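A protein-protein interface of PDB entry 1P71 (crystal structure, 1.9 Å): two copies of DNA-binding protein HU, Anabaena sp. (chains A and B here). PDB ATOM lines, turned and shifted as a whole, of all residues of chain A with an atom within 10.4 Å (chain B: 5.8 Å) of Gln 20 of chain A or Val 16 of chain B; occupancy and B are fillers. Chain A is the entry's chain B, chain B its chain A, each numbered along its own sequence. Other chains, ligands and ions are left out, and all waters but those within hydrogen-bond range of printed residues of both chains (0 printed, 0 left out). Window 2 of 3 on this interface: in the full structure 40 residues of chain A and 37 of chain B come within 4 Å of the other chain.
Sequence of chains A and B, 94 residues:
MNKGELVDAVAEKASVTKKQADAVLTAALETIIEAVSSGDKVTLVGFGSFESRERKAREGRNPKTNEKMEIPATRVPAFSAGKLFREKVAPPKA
Among the printed residues, pairs that only touch across the chains: Val 10 of chain A with Val 24 of chain B, Ala 14 of chain A with Val 24 of chain B, Val 16 of chain A with Val 24 of chain B, Gln 20 of chain A with Val 16 of chain B, Ala 21 of chain A with Val 24 of chain B, Ala 23 of chain A with Ala 14 of chain B, Val 24 of chain A with Val 10 of chain B, Val 24 of chain A with Ala 14 of chain B, Val 24 of chain A with Val 16 of chain B, Val 24 of chain A with Ala 21 of chain B, Val 24 of chain A with Val 24 of chain B, Ala 27 of chain A with Val 10 of chain B and Ala 28 of chain A with Val 10 of chain B.
Printed residues of chain B that touch a printed residue of chain A: Val 10, Ala 14, Val 16, Ala 21 and Val 24.
Of the 22 printed residues of chain A, 9 touch a printed residue of chain B.
Hydrophobic or aromatic side chains of chain A within 4 Å of the printed part of chain B: Val 10, Ala 14, Val 16, Val 24, Ala 27 and Ala 28.
Along chain A the printed residues that touch a printed residue of chain B span positions 10 to 28.
Among the printed residues, no Asp or Glu carboxylate lies within 4 Å of a Lys or Arg side-chain nitrogen of the other chain.
N of Val 16 of chain B sits at hydrogen-bond distance from O of Ala 11 of chain B, 3.1 Å away.
The backbone carbonyl oxygen of Ala 11 of chain A lies within hydrogen-bond range of the backbone NH of Val 16 of chain A (3.1 Å).
Val 10 of chain A touches Val 24 of chain B, and with the chains exchanged Val 24 of chain A touches Val 10 of chain B.
Ala 14 of chain A touches Val 24 of chain B, and with the chains exchanged Val 24 of chain A touches Ala 14 of chain B.
Gln 20 of chain A touches Val 16 of chain B, but with the chains exchanged Val 16 of chain A does not touch Gln 20 of chain B (4.7 Å).
Ala 21 of chain A touches Val 24 of chain B, and with the chains exchanged Val 24 of chain A touches Ala 21 of chain B.
Positions printed for both chains: 10, 11, 12, 14, 15, 16, 17, 18, 20, 21 and 24.
Gln 20 of chain A touches just one residue of chain B: Val 16.
Val 16 of chain B touches just these residues of chain A: Gln 20 and Val 24.
Of chain A, only Ala 23 and Val 24 come within 4 Å of Ala 14 of chain B.
No residue of chain A comes within 4 Å of Thr 17 of chain B.
No residue of chain A comes within 4 Å of Gln 20 of chain B.
Of the printed residues of chain B, Val 24 of chain A touches Val 10 (3.5 Å), Ala 14 (3.8 Å), Val 16 (3.4 Å), Ala 21 (3.99 Å) and Val 24 (3.6 Å).
Printed residues of chain B within 4 Å of Ala 14 of chain A: Val 24.
Printed residues of chain A within 4 Å of Ala 21 of chain B: Val 24.
Leu 25 of chain A touches none of the printed residues of chain B.
Lys 18 of chain B touches none of the printed residues of chain A.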
ATOM      1  N   LEU A   6      15.116  10.442  20.135  1.00  0.00           N
ATOM      2  CA  LEU A   6      14.196  10.398  21.273  1.00  0.00           C
ATOM      3  C   LEU A   6      13.581   8.994  21.426  1.00  0.00           C
ATOM      4  O   LEU A   6      13.484   8.469  22.540  1.00  0.00           O
ATOM      5  CB  LEU A   6      13.097  11.467  21.151  1.00  0.00           C
ATOM      6  CG  LEU A   6      11.943  11.464  22.167  1.00  0.00           C
ATOM      7  CD1 LEU A   6      12.422  11.593  23.608  1.00  0.00           C
ATOM      8  CD2 LEU A   6      10.967  12.571  21.857  1.00  0.00           C
ATOM      9  N   VAL A   7      13.175   8.410  20.301  1.00  0.00           N
ATOM     10  CA  VAL A   7      12.612   7.064  20.261  1.00  0.00           C
ATOM     11  C   VAL A   7      13.604   6.015  20.814  1.00  0.00           C
ATOM     12  O   VAL A   7      13.211   5.131  21.592  1.00  0.00           O
ATOM     13  CB  VAL A   7      12.158   6.698  18.824  1.00  0.00           C
ATOM     14  CG1 VAL A   7      12.172   5.182  18.596  1.00  0.00           C
ATOM     15  CG2 VAL A   7      10.783   7.270  18.538  1.00  0.00           C
ATOM     16  N   ASP A   8      14.878   6.126  20.425  1.00  0.00           N
ATOM     17  CA  ASP A   8      15.917   5.223  20.934  1.00  0.00           C
ATOM     18  C   ASP A   8      15.994   5.332  22.448  1.00  0.00           C
ATOM     19  O   ASP A   8      16.075   4.320  23.134  1.00  0.00           O
ATOM     20  CB  ASP A   8      17.293   5.550  20.343  1.00  0.00           C
ATOM     21  CG  ASP A   8      17.664   4.650  19.187  1.00  0.00           C
ATOM     22  OD1 ASP A   8      17.432   5.073  18.033  1.00  0.00           O
ATOM     23  OD2 ASP A   8      18.192   3.513  19.322  1.00  0.00           O
ATOM     24  N   ALA A   9      15.950   6.565  22.960  1.00  0.00           N
ATOM     25  CA  ALA A   9      16.117   6.826  24.393  1.00  0.00           C
ATOM     26  C   ALA A   9      14.943   6.288  25.208  1.00  0.00           C
ATOM     27  O   ALA A   9      15.110   5.827  26.343  1.00  0.00           O
ATOM     28  CB  ALA A   9      16.299   8.331  24.646  1.00  0.00           C
ATOM     29  N   VAL A  10      13.760   6.331  24.600  1.00  0.00           N
ATOM     30  CA  VAL A  10      12.512   5.933  25.254  1.00  0.00           C
ATOM     31  C   VAL A  10      12.193   4.429  25.154  1.00  0.00           C
ATOM     32  O   VAL A  10      11.489   3.881  26.016  1.00  0.00           O
ATOM     33  CB  VAL A  10      11.335   6.761  24.730  1.00  0.00           C
ATOM     34  CG1 VAL A  10      10.017   6.200  25.223  1.00  0.00           C
ATOM     35  CG2 VAL A  10      11.477   8.206  25.174  1.00  0.00           C
ATOM     36  N   ALA A  11      12.686   3.774  24.103  1.00  0.00           N
ATOM     37  CA  ALA A  11      12.608   2.312  24.023  1.00  0.00           C
ATOM     38  C   ALA A  11      13.368   1.736  25.214  1.00  0.00           C
ATOM     39  O   ALA A  11      12.959   0.733  25.802  1.00  0.00           O
ATOM     40  CB  ALA A  11      13.203   1.811  22.710  1.00  0.00           C
ATOM     41  N   GLU A  12      14.461   2.404  25.580  1.00  0.00           N
ATOM     42  CA  GLU A  12      15.362   1.932  26.629  1.00  0.00           C
ATOM     43  C   GLU A  12      14.759   2.034  28.040  1.00  0.00           C
ATOM     44  O   GLU A  12      14.721   1.038  28.782  1.00  0.00           O
ATOM     45  CB  GLU A  12      16.701   2.673  26.542  1.00  0.00           C
ATOM     46  CG  GLU A  12      17.539   2.276  25.334  1.00  0.00           C
ATOM     47  N   ALA A  14      11.599   2.469  28.971  1.00  0.00           N
ATOM     48  CA  ALA A  14      10.307   1.784  29.151  1.00  0.00           C
ATOM     49  C   ALA A  14      10.421   0.255  29.005  1.00  0.00           C
ATOM     50  O   ALA A  14       9.496  -0.519  29.398  1.00  0.00           O
ATOM     51  CB  ALA A  14       9.226   2.373  28.195  1.00  0.00           C
ATOM     52  N   SER A  15      11.574  -0.176  28.470  1.00  0.00           N
ATOM     53  CA  SER A  15      11.816  -1.588  28.164  1.00  0.00           C
ATOM     54  C   SER A  15      10.877  -2.178  27.092  1.00  0.00           C
ATOM     55  O   SER A  15      10.259  -3.288  27.313  1.00  0.00           O
ATOM     56  CB  SER A  15      11.823  -2.442  29.442  1.00  0.00           C
ATOM     57  OG  SER A  15      13.146  -2.651  29.898  1.00  0.00           O
ATOM     58  N   VAL A  16      10.789  -1.427  25.920  1.00  0.00           N
ATOM     59  CA  VAL A  16      10.123  -1.965  24.730  1.00  0.00           C
ATOM     60  C   VAL A  16      11.182  -2.148  23.600  1.00  0.00           C
ATOM     61  O   VAL A  16      12.480  -1.985  23.842  1.00  0.00           O
ATOM     62  CB  VAL A  16       8.907  -1.009  24.276  1.00  0.00           C
ATOM     63  CG1 VAL A  16       7.809  -0.966  25.353  1.00  0.00           C
ATOM     64  CG2 VAL A  16       9.376   0.427  23.887  1.00  0.00           C
ATOM     65  N   THR A  17      10.618  -2.489  22.370  1.00  0.00           N
ATOM     66  CA  THR A  17      11.304  -2.310  21.046  1.00  0.00           C
ATOM     67  C   THR A  17      11.376  -0.816  20.627  1.00  0.00           C
ATOM     68  O   THR A  17      10.651   0.062  21.191  1.00  0.00           O
ATOM     69  CB  THR A  17      10.539  -3.061  19.867  1.00  0.00           C
ATOM     70  OG1 THR A  17      10.914  -2.483  18.600  1.00  0.00           O
ATOM     71  CG2 THR A  17       9.009  -2.726  19.855  1.00  0.00           C
ATOM     72  N   LYS A  18      12.240  -0.551  19.622  1.00  0.00           N
ATOM     73  CA  LYS A  18      12.308   0.771  18.965  1.00  0.00           C
ATOM     74  C   LYS A  18      11.029   1.057  18.156  1.00  0.00           C
ATOM     75  O   LYS A  18      10.544   2.199  18.087  1.00  0.00           O
ATOM     76  CB  LYS A  18      13.523   0.821  18.026  1.00  0.00           C
ATOM     77  CG  LYS A  18      14.890   0.927  18.762  1.00  0.00           C
ATOM     78  N   LYS A  19      10.499  -0.002  17.549  1.00  0.00           N
ATOM     79  CA  LYS A  19       9.287   0.044  16.741  1.00  0.00           C
ATOM     80  C   LYS A  19       8.040   0.403  17.549  1.00  0.00           C
ATOM     81  O   LYS A  19       7.045   0.890  16.916  1.00  0.00           O
ATOM     82  CB  LYS A  19       9.085  -1.314  16.038  1.00  0.00           C
ATOM     83  CG  LYS A  19       8.223  -1.255  14.767  1.00  0.00           C
ATOM     84  CD  LYS A  19       8.135  -2.617  14.076  1.00  0.00           C
ATOM     85  CE  LYS A  19       7.002  -3.507  14.631  1.00  0.00           C
ATOM     86  NZ  LYS A  19       5.783  -2.730  15.019  1.00  0.00           N
ATOM     87  N   GLN A  20       8.086   0.160  18.941  1.00  0.00           N
ATOM     88  CA  GLN A  20       6.896   0.468  19.752  1.00  0.00           C
ATOM     89  C   GLN A  20       7.022   1.874  20.311  1.00  0.00           C
ATOM     90  O   GLN A  20       6.042   2.624  20.392  1.00  0.00           O
ATOM     91  CB  GLN A  20       6.720  -0.525  20.912  1.00  0.00           C
ATOM     92  CG  GLN A  20       5.795  -1.826  20.487  1.00  0.00           C
ATOM     93  CD  GLN A  20       5.989  -2.845  21.658  1.00  0.00           C
ATOM     94  OE1 GLN A  20       5.445  -3.964  21.557  1.00  0.00           O
ATOM     95  NE2 GLN A  20       6.785  -2.479  22.760  1.00  0.00           N
ATOM     96  N   ALA A  21       8.238   2.228  20.720  1.00  0.00           N
ATOM     97  CA  ALA A  21       8.502   3.579  21.157  1.00  0.00           C
ATOM     98  C   ALA A  21       8.040   4.504  20.031  1.00  0.00           C
ATOM     99  O   ALA A  21       7.210   5.399  20.259  1.00  0.00           O
ATOM    100  CB  ALA A  21       9.985   3.768  21.454  1.00  0.00           C
ATOM    101  N   ASP A  22       8.512   4.228  18.810  1.00  0.00           N
ATOM    102  CA  ASP A  22       8.209   5.070  17.636  1.00  0.00           C
ATOM    103  C   ASP A  22       6.708   5.151  17.301  1.00  0.00           C
ATOM    104  O   ASP A  22       6.188   6.240  17.059  1.00  0.00           O
ATOM    105  CB  ASP A  22       9.006   4.602  16.415  1.00  0.00           C
ATOM    106  CG  ASP A  22       8.608   5.330  15.149  1.00  0.00           C
ATOM    107  OD1 ASP A  22       7.789   4.798  14.365  1.00  0.00           O
ATOM    108  OD2 ASP A  22       9.049   6.452  14.860  1.00  0.00           O
ATOM    109  N   ALA A  23       6.032   4.004  17.288  1.00  0.00           N
ATOM    110  CA  ALA A  23       4.598   3.943  16.995  1.00  0.00           C
ATOM    111  C   ALA A  23       3.757   4.616  18.082  1.00  0.00           C
ATOM    112  O   ALA A  23       2.733   5.244  17.786  1.00  0.00           O
ATOM    113  CB  ALA A  23       4.151   2.476  16.772  1.00  0.00           C
ATOM    114  N   VAL A  24       4.200   4.495  19.336  1.00  0.00           N
ATOM    115  CA  VAL A  24       3.575   5.225  20.446  1.00  0.00           C
ATOM    116  C   VAL A  24       3.826   6.725  20.318  1.00  0.00           C
ATOM    117  O   VAL A  24       2.884   7.512  20.418  1.00  0.00           O
ATOM    118  CB  VAL A  24       4.042   4.712  21.834  1.00  0.00           C
ATOM    119  CG1 VAL A  24       3.691   5.711  22.956  1.00  0.00           C
ATOM    120  CG2 VAL A  24       3.450   3.356  22.131  1.00  0.00           C
ATOM    121  N   LEU A  25       5.083   7.124  20.102  1.00  0.00           N
ATOM    122  CA  LEU A  25       5.413   8.547  19.990  1.00  0.00           C
ATOM    123  C   LEU A  25       4.664   9.193  18.829  1.00  0.00           C
ATOM    124  O   LEU A  25       4.001  10.217  19.016  1.00  0.00           O
ATOM    125  CB  LEU A  25       6.924   8.800  19.894  1.00  0.00           C
ATOM    126  CG  LEU A  25       7.339  10.283  19.822  1.00  0.00           C
ATOM    127  CD1 LEU A  25       6.804  11.097  21.012  1.00  0.00           C
ATOM    128  CD2 LEU A  25       8.858  10.452  19.686  1.00  0.00           C
ATOM    129  N   THR A  26       4.737   8.563  17.651  1.00  0.00           N
ATOM    130  CA  THR A  26       4.057   9.060  16.456  1.00  0.00           C
ATOM    131  C   THR A  26       2.574   9.275  16.749  1.00  0.00           C
ATOM    132  O   THR A  26       2.014  10.332  16.451  1.00  0.00           O
ATOM    133  CB  THR A  26       4.239   8.061  15.266  1.00  0.00           C
ATOM    134  OG1 THR A  26       5.634   7.933  14.935  1.00  0.00           O
ATOM    135  CG2 THR A  26       3.644   8.634  13.999  1.00  0.00           C
ATOM    136  N   ALA A  27       1.948   8.265  17.348  1.00  0.00           N
ATOM    137  CA  ALA A  27       0.525   8.315  17.633  1.00  0.00           C
ATOM    138  C   ALA A  27       0.233   9.486  18.557  1.00  0.00           C
ATOM    139  O   ALA A  27      -0.682  10.261  18.317  1.00  0.00           O
ATOM    140  CB  ALA A  27       0.046   7.009  18.233  1.00  0.00           C
ATOM    141  N   ALA A  28       1.038   9.624  19.599  1.00  0.00           N
ATOM    142  CA  ALA A  28       0.858  10.683  20.576  1.00  0.00           C
ATOM    143  C   ALA A  28       0.919  12.091  19.969  1.00  0.00           C
ATOM    144  O   ALA A  28       0.096  12.942  20.312  1.00  0.00           O
ATOM    145  CB  ALA A  28       1.876  10.512  21.720  1.00  0.00           C
ATOM    146  N   VAL B  10      -3.665   6.707  22.125  1.00  0.00           N
ATOM    147  CA  VAL B  10      -2.385   6.202  21.619  1.00  0.00           C
ATOM    148  C   VAL B  10      -2.350   4.670  21.623  1.00  0.00           C
ATOM    149  O   VAL B  10      -2.048   4.034  20.601  1.00  0.00           O
ATOM    150  CB  VAL B  10      -1.203   6.771  22.430  1.00  0.00           C
ATOM    151  CG1 VAL B  10       0.093   6.097  22.036  1.00  0.00           C
ATOM    152  CG2 VAL B  10      -1.100   8.276  22.217  1.00  0.00           C
ATOM    153  N   ALA B  11      -2.673   4.088  22.775  1.00  0.00           N
ATOM    154  CA  ALA B  11      -2.731   2.636  22.923  1.00  0.00           C
ATOM    155  C   ALA B  11      -3.567   2.040  21.798  1.00  0.00           C
ATOM    156  O   ALA B  11      -3.203   1.029  21.221  1.00  0.00           O
ATOM    157  CB  ALA B  11      -3.312   2.274  24.272  1.00  0.00           C
ATOM    158  N   GLU B  12      -4.673   2.706  21.476  1.00  0.00           N
ATOM    159  CA  GLU B  12      -5.543   2.322  20.370  1.00  0.00           C
ATOM    160  C   GLU B  12      -4.891   2.494  18.985  1.00  0.00           C
ATOM    161  O   GLU B  12      -4.987   1.598  18.136  1.00  0.00           O
ATOM    162  CB  GLU B  12      -6.858   3.109  20.441  1.00  0.00           C
ATOM    163  N   ALA B  14      -1.585   2.875  18.186  1.00  0.00           N
ATOM    164  CA  ALA B  14      -0.304   2.167  18.041  1.00  0.00           C
ATOM    165  C   ALA B  14      -0.390   0.678  18.365  1.00  0.00           C
ATOM    166  O   ALA B  14       0.588  -0.063  18.184  1.00  0.00           O
ATOM    167  CB  ALA B  14       0.760   2.834  18.914  1.00  0.00           C
ATOM    168  N   SER B  15      -1.569   0.251  18.829  1.00  0.00           N
ATOM    169  CA  SER B  15      -1.837  -1.129  19.254  1.00  0.00           C
ATOM    170  C   SER B  15      -0.878  -1.624  20.354  1.00  0.00           C
ATOM    171  O   SER B  15      -0.386  -2.834  20.275  1.00  0.00           O
ATOM    172  CB  SER B  15      -1.878  -2.084  18.053  1.00  0.00           C
ATOM    173  OG  SER B  15      -2.866  -1.681  17.117  1.00  0.00           O
ATOM    174  N   VAL B  16      -0.616  -0.674  21.370  1.00  0.00           N
ATOM    175  CA  VAL B  16       0.071  -1.080  22.608  1.00  0.00           C
ATOM    176  C   VAL B  16      -0.827  -0.901  23.846  1.00  0.00           C
ATOM    177  O   VAL B  16      -1.846  -0.075  23.806  1.00  0.00           O
ATOM    178  CB  VAL B  16       1.391  -0.323  22.799  1.00  0.00           C
ATOM    179  CG1 VAL B  16       2.253  -0.433  21.535  1.00  0.00           C
ATOM    180  CG2 VAL B  16       1.126   1.127  23.187  1.00  0.00           C
ATOM    181  N   THR B  17      -0.460  -1.683  24.929  1.00  0.00           N
ATOM    182  CA  THR B  17      -1.188  -1.654  26.205  1.00  0.00           C
ATOM    183  C   THR B  17      -1.326  -0.210  26.667  1.00  0.00           C
ATOM    184  O   THR B  17      -0.443   0.612  26.386  1.00  0.00           O
ATOM    185  CB  THR B  17      -0.455  -2.486  27.284  1.00  0.00           C
ATOM    186  OG1 THR B  17      -0.497  -3.878  26.931  1.00  0.00           O
ATOM    187  CG2 THR B  17      -1.224  -2.464  28.614  1.00  0.00           C
ATOM    188  N   LYS B  18      -2.434   0.091  27.363  1.00  0.00           N
ATOM    189  CA  LYS B  18      -2.619   1.392  28.018  1.00  0.00           C
ATOM    190  C   LYS B  18      -1.472   1.686  29.000  1.00  0.00           C
ATOM    191  O   LYS B  18      -1.052   2.839  29.150  1.00  0.00           O
ATOM    192  CB  LYS B  18      -3.986   1.460  28.724  1.00  0.00           C
ATOM    193  CG  LYS B  18      -5.046   2.254  27.942  1.00  0.00           C
ATOM    194  CD  LYS B  18      -6.449   1.950  28.482  1.00  0.00           C
ATOM    195  N   GLN B  20       1.659   0.604  28.423  1.00  0.00           N
ATOM    196  CA  GLN B  20       2.845   0.782  27.582  1.00  0.00           C
ATOM    197  C   GLN B  20       2.819   2.124  26.923  1.00  0.00           C
ATOM    198  O   GLN B  20       3.858   2.786  26.794  1.00  0.00           O
ATOM    199  CB  GLN B  20       2.920  -0.285  26.491  1.00  0.00           C
ATOM    200  CG  GLN B  20       3.424  -1.662  26.976  1.00  0.00           C
ATOM    201  CD  GLN B  20       3.305  -2.672  25.841  1.00  0.00           C
ATOM    202  OE1 GLN B  20       3.994  -3.862  26.083  1.00  0.00           O
ATOM    203  NE2 GLN B  20       2.408  -2.237  24.609  1.00  0.00           N
ATOM    204  N   ALA B  21       1.628   2.539  26.469  1.00  0.00           N
ATOM    205  CA  ALA B  21       1.507   3.870  25.912  1.00  0.00           C
ATOM    206  C   ALA B  21       1.876   4.829  27.024  1.00  0.00           C
ATOM    207  O   ALA B  21       2.705   5.749  26.820  1.00  0.00           O
ATOM    208  CB  ALA B  21       0.109   4.151  25.451  1.00  0.00           C
ATOM    209  N   VAL B  24       5.773   4.516  27.668  1.00  0.00           N
ATOM    210  CA  VAL B  24       6.565   5.154  26.622  1.00  0.00           C
ATOM    211  C   VAL B  24       6.328   6.678  26.590  1.00  0.00           C
ATOM    212  O   VAL B  24       7.269   7.461  26.433  1.00  0.00           O
ATOM    213  CB  VAL B  24       6.294   4.504  25.231  1.00  0.00           C
ATOM    214  CG1 VAL B  24       7.032   5.256  24.114  1.00  0.00           C
ATOM    215  CG2 VAL B  24       6.679   3.030  25.233  1.00  0.00           C
